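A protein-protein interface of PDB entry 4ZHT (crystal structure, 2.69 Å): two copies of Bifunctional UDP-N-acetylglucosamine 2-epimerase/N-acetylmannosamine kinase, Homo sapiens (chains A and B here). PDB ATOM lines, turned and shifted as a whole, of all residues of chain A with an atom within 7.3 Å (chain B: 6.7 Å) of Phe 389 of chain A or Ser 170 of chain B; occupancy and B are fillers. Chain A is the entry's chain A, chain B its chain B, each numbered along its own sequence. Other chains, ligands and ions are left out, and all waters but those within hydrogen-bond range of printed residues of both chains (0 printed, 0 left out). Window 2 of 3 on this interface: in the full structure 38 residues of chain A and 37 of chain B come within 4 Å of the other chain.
Met 171 of chain A touches Cys 172 of chain B (CG to SG, 3.95 Å).
CG of Met 171 of chain B touches SG of Cys 172 of chain A, 3.8 Å away.
CD2 of His 167 of chain B touches CB of Cys 388 of chain A, 3.5 Å away.
Ser 170 of chain A touches its own counterpart, Ser 170 of chain B.
Ser 170 of chain A touches Cys 172 of chain B, and with the chains exchanged Cys 172 of chain A touches Ser 170 of chain B.
Met 171 of chain A touches Cys 172 of chain B, and with the chains exchanged Cys 172 of chain A touches Met 171 of chain B.
Positions printed for both chains: 169, 170, 171, 172, 173 and 387.
Of the 7 pairs that touch across the chains among the printed residues, 5 have their exchanged pair printed and touching as well.
Hydrophobic or aromatic side chains of chain A within 4 Å of the printed part of chain B: Met 171.
Of the 10 printed residues of chain B, 4 touch a printed residue of chain A.
Hydrophobic or aromatic side chains of chain B within 4 Å of the printed part of chain A: His 167 and Met 171.
The backbone NH (N) of Phe 387 of chain A sits at hydrogen-bond distance from the backbone carbonyl oxygen (O) of Cys 172 of chain A (3.1 Å).
O of Gln 166 of chain B is in hydrogen-bond range of OG of Ser 170 of chain B (3.4 Å).
O of Cys 172 of chain B lies within hydrogen-bond range of N of Phe 387 of chain B (3.2 Å).
Of the printed residues of chain B, Cys 172 of chain A touches Ser 170 and Met 171.
Phe 389 of chain A touches one residue of chain B.
Of the printed residues of chain A, His 167 of chain B touches Cys 388.
Glu 173 of chain B touches none of the printed residues of chain A.
The backbone carbonyl oxygen (O) of Ser 170 of chain B sits close to the backbone carbonyl oxygen (O) of Ser 170 of chain A (2.9 Å).
The side-chain sulfur of Cys 172 of chain B lies within hydrogen-bond range of the backbone carbonyl oxygen of Ser 170 of chain A, 3.5 Å away.
SG of Cys 172 of chain A sits at hydrogen-bond distance from O of Ser 170 of chain B, at 3.5 Å.
The side-chain hydroxyl of Ser 170 of chain B sits at hydrogen-bond distance from the backbone carbonyl oxygen of Phe 389 of chain A (2.8 Å).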
ATOM      1  N   ILE A 169       7.099   2.072  13.210  1.00  0.00           N
ATOM      2  CA  ILE A 169       7.756   3.287  12.740  1.00  0.00           C
ATOM      3  C   ILE A 169       8.971   3.599  13.616  1.00  0.00           C
ATOM      4  O   ILE A 169      10.007   3.990  13.079  1.00  0.00           O
ATOM      5  CB  ILE A 169       6.792   4.499  12.648  1.00  0.00           C
ATOM      6  CG1 ILE A 169       5.730   4.219  11.588  1.00  0.00           C
ATOM      7  CG2 ILE A 169       7.544   5.787  12.276  1.00  0.00           C
ATOM      8  CD1 ILE A 169       4.618   5.243  11.524  1.00  0.00           C
ATOM      9  N   SER A 170       8.851   3.437  14.937  1.00  0.00           N
ATOM     10  CA  SER A 170      10.007   3.616  15.844  1.00  0.00           C
ATOM     11  C   SER A 170      11.124   2.616  15.556  1.00  0.00           C
ATOM     12  O   SER A 170      12.290   2.951  15.672  1.00  0.00           O
ATOM     13  CB  SER A 170       9.625   3.469  17.322  1.00  0.00           C
ATOM     14  OG  SER A 170       9.043   4.651  17.843  1.00  0.00           O
ATOM     15  N   MET A 171      10.763   1.411  15.151  1.00  0.00           N
ATOM     16  CA  MET A 171      11.759   0.404  14.764  1.00  0.00           C
ATOM     17  C   MET A 171      12.305   0.643  13.370  1.00  0.00           C
ATOM     18  O   MET A 171      12.913  -0.269  12.792  1.00  0.00           O
ATOM     19  CB  MET A 171      11.158  -1.002  14.935  1.00  0.00           C
ATOM     20  CG  MET A 171      11.183  -1.455  16.391  1.00  0.00           C
ATOM     21  SD  MET A 171      10.394  -3.262  16.606  1.00  0.00           S
ATOM     22  CE  MET A 171       8.634  -3.086  15.890  1.00  0.00           C
ATOM     23  N   CYS A 172      12.109   1.854  12.826  1.00  0.00           N
ATOM     24  CA  CYS A 172      12.632   2.290  11.524  1.00  0.00           C
ATOM     25  C   CYS A 172      12.032   1.617  10.292  1.00  0.00           C
ATOM     26  O   CYS A 172      12.703   1.497   9.271  1.00  0.00           O
ATOM     27  CB  CYS A 172      14.159   2.194  11.478  1.00  0.00           C
ATOM     28  SG  CYS A 172      14.980   3.023  12.839  1.00  0.00           S
ATOM     29  N   GLU A 173      10.771   1.205  10.361  1.00  0.00           N
ATOM     30  CA  GLU A 173      10.079   0.712   9.167  1.00  0.00           C
ATOM     31  C   GLU A 173       9.473   1.863   8.370  1.00  0.00           C
ATOM     32  O   GLU A 173       9.137   2.914   8.921  1.00  0.00           O
ATOM     33  CB  GLU A 173       9.017  -0.347   9.512  1.00  0.00           C
ATOM     34  CG  GLU A 173       9.601  -1.679  10.014  1.00  0.00           C
ATOM     35  CD  GLU A 173      10.483  -2.393   8.988  1.00  0.00           C
ATOM     36  OE1 GLU A 173      10.323  -2.167   7.772  1.00  0.00           O
ATOM     37  OE2 GLU A 173      11.360  -3.182   9.408  1.00  0.00           O
ATOM     38  N   HIS A 175       6.873   3.922   6.675  1.00  0.00           N
ATOM     39  CA  HIS A 175       5.454   4.119   6.946  1.00  0.00           C
ATOM     40  C   HIS A 175       4.558   3.832   5.720  1.00  0.00           C
ATOM     41  O   HIS A 175       3.434   3.341   5.877  1.00  0.00           O
ATOM     42  CB  HIS A 175       5.199   5.491   7.591  1.00  0.00           C
ATOM     43  CG  HIS A 175       5.430   6.675   6.706  1.00  0.00           C
ATOM     44  ND1 HIS A 175       4.397   7.338   6.081  1.00  0.00           N
ATOM     45  CD2 HIS A 175       6.552   7.389   6.439  1.00  0.00           C
ATOM     46  CE1 HIS A 175       4.879   8.384   5.430  1.00  0.00           C
ATOM     47  NE2 HIS A 175       6.183   8.438   5.631  1.00  0.00           N
ATOM     48  N   LYS A 386      14.975   1.276   5.059  1.00  0.00           N
ATOM     49  CA  LYS A 386      15.126   1.373   6.506  1.00  0.00           C
ATOM     50  C   LYS A 386      15.356   2.837   6.856  1.00  0.00           C
ATOM     51  O   LYS A 386      16.420   3.389   6.579  1.00  0.00           O
ATOM     52  CB  LYS A 386      16.315   0.530   6.972  1.00  0.00           C
ATOM     53  CG  LYS A 386      16.258  -0.928   6.547  1.00  0.00           C
ATOM     54  CD  LYS A 386      15.481  -1.739   7.547  1.00  0.00           C
ATOM     55  CE  LYS A 386      14.633  -2.774   6.867  1.00  0.00           C
ATOM     56  NZ  LYS A 386      15.026  -4.116   7.310  1.00  0.00           N
ATOM     57  N   PHE A 387      14.335   3.456   7.438  1.00  0.00           N
ATOM     58  CA  PHE A 387      14.350   4.877   7.768  1.00  0.00           C
ATOM     59  C   PHE A 387      15.133   5.173   9.050  1.00  0.00           C
ATOM     60  O   PHE A 387      14.569   5.245  10.137  1.00  0.00           O
ATOM     61  CB  PHE A 387      12.908   5.389   7.862  1.00  0.00           C
ATOM     62  CG  PHE A 387      12.230   5.608   6.527  1.00  0.00           C
ATOM     63  CD1 PHE A 387      12.950   5.791   5.326  1.00  0.00           C
ATOM     64  CD2 PHE A 387      10.847   5.725   6.485  1.00  0.00           C
ATOM     65  CE1 PHE A 387      12.290   6.038   4.127  1.00  0.00           C
ATOM     66  CE2 PHE A 387      10.185   5.985   5.289  1.00  0.00           C
ATOM     67  CZ  PHE A 387      10.903   6.136   4.107  1.00  0.00           C
ATOM     68  N   CYS A 388      16.448   5.328   8.900  1.00  0.00           N
ATOM     69  CA  CYS A 388      17.349   5.617  10.025  1.00  0.00           C
ATOM     70  C   CYS A 388      17.533   7.138  10.211  1.00  0.00           C
ATOM     71  O   CYS A 388      18.471   7.742   9.683  1.00  0.00           O
ATOM     72  CB  CYS A 388      18.711   4.875   9.870  1.00  0.00           C
ATOM     73  SG  CYS A 388      18.775   3.092  10.313  1.00  0.00           S
ATOM     74  N   PHE A 389      16.596   7.748  10.937  1.00  0.00           N
ATOM     75  CA  PHE A 389      16.764   9.100  11.463  1.00  0.00           C
ATOM     76  C   PHE A 389      17.814   9.085  12.577  1.00  0.00           C
ATOM     77  O   PHE A 389      17.623   8.373  13.569  1.00  0.00           O
ATOM     78  CB  PHE A 389      15.440   9.625  12.062  1.00  0.00           C
ATOM     79  CG  PHE A 389      14.321   9.847  11.054  1.00  0.00           C
ATOM     80  CD1 PHE A 389      14.113  11.120  10.503  1.00  0.00           C
ATOM     81  CD2 PHE A 389      13.444   8.804  10.680  1.00  0.00           C
ATOM     82  CE1 PHE A 389      13.090  11.346   9.586  1.00  0.00           C
ATOM     83  CE2 PHE A 389      12.419   9.032   9.762  1.00  0.00           C
ATOM     84  CZ  PHE A 389      12.242  10.302   9.217  1.00  0.00           C
ATOM     85  N   PRO A 390      18.925   9.853  12.414  1.00  0.00           N
ATOM     86  CA  PRO A 390      19.789  10.175  13.555  1.00  0.00           C
ATOM     87  C   PRO A 390      19.343  11.470  14.258  1.00  0.00           C
ATOM     88  O   PRO A 390      19.472  11.602  15.481  1.00  0.00           O
ATOM     89  CB  PRO A 390      21.186  10.348  12.910  1.00  0.00           C
ATOM     90  CG  PRO A 390      21.001  10.195  11.430  1.00  0.00           C
ATOM     91  CD  PRO A 390      19.537  10.347  11.164  1.00  0.00           C
ATOM     92  N   GLU B 165      26.283   2.636  16.006  1.00  0.00           N
ATOM     93  CA  GLU B 165      25.728   2.688  17.354  1.00  0.00           C
ATOM     94  C   GLU B 165      24.388   3.418  17.355  1.00  0.00           C
ATOM     95  O   GLU B 165      23.439   2.966  17.992  1.00  0.00           O
ATOM     96  CB  GLU B 165      26.704   3.374  18.318  1.00  0.00           C
ATOM     97  CG  GLU B 165      26.179   3.563  19.740  1.00  0.00           C
ATOM     98  CD  GLU B 165      27.206   4.157  20.684  1.00  0.00           C
ATOM     99  OE1 GLU B 165      27.939   5.111  20.293  1.00  0.00           O
ATOM    100  OE2 GLU B 165      27.276   3.668  21.833  1.00  0.00           O
ATOM    101  N   GLN B 166      24.317   4.561  16.667  1.00  0.00           N
ATOM    102  CA  GLN B 166      23.074   5.351  16.635  1.00  0.00           C
ATOM    103  C   GLN B 166      21.970   4.607  15.889  1.00  0.00           C
ATOM    104  O   GLN B 166      20.813   4.655  16.297  1.00  0.00           O
ATOM    105  CB  GLN B 166      23.288   6.774  16.074  1.00  0.00           C
ATOM    106  CG  GLN B 166      24.188   7.662  16.985  1.00  0.00           C
ATOM    107  CD  GLN B 166      23.522   8.155  18.282  1.00  0.00           C
ATOM    108  OE1 GLN B 166      22.699   7.465  18.901  1.00  0.00           O
ATOM    109  NE2 GLN B 166      23.925   9.345  18.728  1.00  0.00           N
ATOM    110  N   HIS B 167      22.332   3.876  14.841  1.00  0.00           N
ATOM    111  CA  HIS B 167      21.349   3.062  14.141  1.00  0.00           C
ATOM    112  C   HIS B 167      20.726   2.007  15.050  1.00  0.00           C
ATOM    113  O   HIS B 167      19.512   1.851  15.048  1.00  0.00           O
ATOM    114  CB  HIS B 167      21.948   2.411  12.891  1.00  0.00           C
ATOM    115  CG  HIS B 167      22.248   3.377  11.792  1.00  0.00           C
ATOM    116  ND1 HIS B 167      23.193   3.131  10.820  1.00  0.00           N
ATOM    117  CD2 HIS B 167      21.739   4.606  11.527  1.00  0.00           C
ATOM    118  CE1 HIS B 167      23.243   4.160   9.993  1.00  0.00           C
ATOM    119  NE2 HIS B 167      22.371   5.069  10.403  1.00  0.00           N
ATOM    120  N   LEU B 168      21.554   1.287  15.812  1.00  0.00           N
ATOM    121  CA  LEU B 168      21.054   0.299  16.780  1.00  0.00           C
ATOM    122  C   LEU B 168      20.119   0.953  17.807  1.00  0.00           C
ATOM    123  O   LEU B 168      19.049   0.412  18.094  1.00  0.00           O
ATOM    124  CB  LEU B 168      22.203  -0.420  17.489  1.00  0.00           C
ATOM    125  CG  LEU B 168      23.100  -1.356  16.660  1.00  0.00           C
ATOM    126  CD1 LEU B 168      24.347  -1.778  17.419  1.00  0.00           C
ATOM    127  CD2 LEU B 168      22.356  -2.597  16.215  1.00  0.00           C
ATOM    128  N   ILE B 169      20.493   2.133  18.320  1.00  0.00           N
ATOM    129  CA  ILE B 169      19.650   2.848  19.278  1.00  0.00           C
ATOM    130  C   ILE B 169      18.358   3.310  18.595  1.00  0.00           C
ATOM    131  O   ILE B 169      17.295   3.201  19.198  1.00  0.00           O
ATOM    132  CB  ILE B 169      20.386   4.030  19.964  1.00  0.00           C
ATOM    133  CG1 ILE B 169      21.533   3.489  20.818  1.00  0.00           C
ATOM    134  CG2 ILE B 169      19.431   4.842  20.851  1.00  0.00           C
ATOM    135  CD1 ILE B 169      22.436   4.555  21.395  1.00  0.00           C
ATOM    136  N   SER B 170      18.444   3.810  17.356  1.00  0.00           N
ATOM    137  CA  SER B 170      17.236   4.183  16.582  1.00  0.00           C
ATOM    138  C   SER B 170      16.339   2.983  16.330  1.00  0.00           C
ATOM    139  O   SER B 170      15.128   3.111  16.318  1.00  0.00           O
ATOM    140  CB  SER B 170      17.572   4.801  15.223  1.00  0.00           C
ATOM    141  OG  SER B 170      17.917   6.165  15.335  1.00  0.00           O
ATOM    142  N   MET B 171      16.939   1.805  16.141  1.00  0.00           N
ATOM    143  CA  MET B 171      16.165   0.573  15.954  1.00  0.00           C
ATOM    144  C   MET B 171      15.638   0.020  17.271  1.00  0.00           C
ATOM    145  O   MET B 171      15.234  -1.145  17.325  1.00  0.00           O
ATOM    146  CB  MET B 171      17.007  -0.443  15.161  1.00  0.00           C
ATOM    147  CG  MET B 171      16.960  -0.119  13.671  1.00  0.00           C
ATOM    148  SD  MET B 171      17.866  -1.412  12.519  1.00  0.00           S
ATOM    149  CE  MET B 171      19.709  -1.356  13.390  1.00  0.00           C
ATOM    150  N   CYS B 172      15.627   0.845  18.323  1.00  0.00           N
ATOM    151  CA  CYS B 172      15.091   0.516  19.655  1.00  0.00           C
ATOM    152  C   CYS B 172      15.865  -0.552  20.445  1.00  0.00           C
ATOM    153  O   CYS B 172      15.275  -1.233  21.268  1.00  0.00           O
ATOM    154  CB  CYS B 172      13.607   0.150  19.584  1.00  0.00           C
ATOM    155  SG  CYS B 172      12.600   1.377  18.757  1.00  0.00           S
ATOM    156  N   GLU B 173      17.178  -0.652  20.247  1.00  0.00           N
ATOM    157  CA  GLU B 173      18.002  -1.491  21.115  1.00  0.00           C
ATOM    158  C   GLU B 173      18.405  -0.729  22.395  1.00  0.00           C
ATOM    159  O   GLU B 173      18.535   0.496  22.404  1.00  0.00           O
ATOM    160  CB  GLU B 173      19.228  -2.036  20.373  1.00  0.00           C
ATOM    161  CG  GLU B 173      18.879  -3.058  19.268  1.00  0.00           C
ATOM    162  CD  GLU B 173      18.191  -4.318  19.784  1.00  0.00           C
ATOM    163  OE1 GLU B 173      18.354  -4.656  20.979  1.00  0.00           O
ATOM    164  OE2 GLU B 173      17.460  -4.959  19.011  1.00  0.00           O
ATOM    165  N   PHE B 387      13.394  -0.708  23.744  1.00  0.00           N
ATOM    166  CA  PHE B 387      13.107   0.661  24.129  1.00  0.00           C
ATOM    167  C   PHE B 387      12.225   1.393  23.114  1.00  0.00           C
ATOM    168  O   PHE B 387      12.716   2.078  22.206  1.00  0.00           O
ATOM    169  CB  PHE B 387      14.427   1.392  24.338  1.00  0.00           C
ATOM    170  CG  PHE B 387      15.116   1.076  25.641  1.00  0.00           C
ATOM    171  CD1 PHE B 387      14.431   0.555  26.761  1.00  0.00           C
ATOM    172  CD2 PHE B 387      16.455   1.434  25.798  1.00  0.00           C
ATOM    173  CE1 PHE B 387      15.094   0.359  27.966  1.00  0.00           C
ATOM    174  CE2 PHE B 387      17.121   1.240  27.007  1.00  0.00           C
ATOM    175  CZ  PHE B 387      16.442   0.694  28.091  1.00  0.00           C
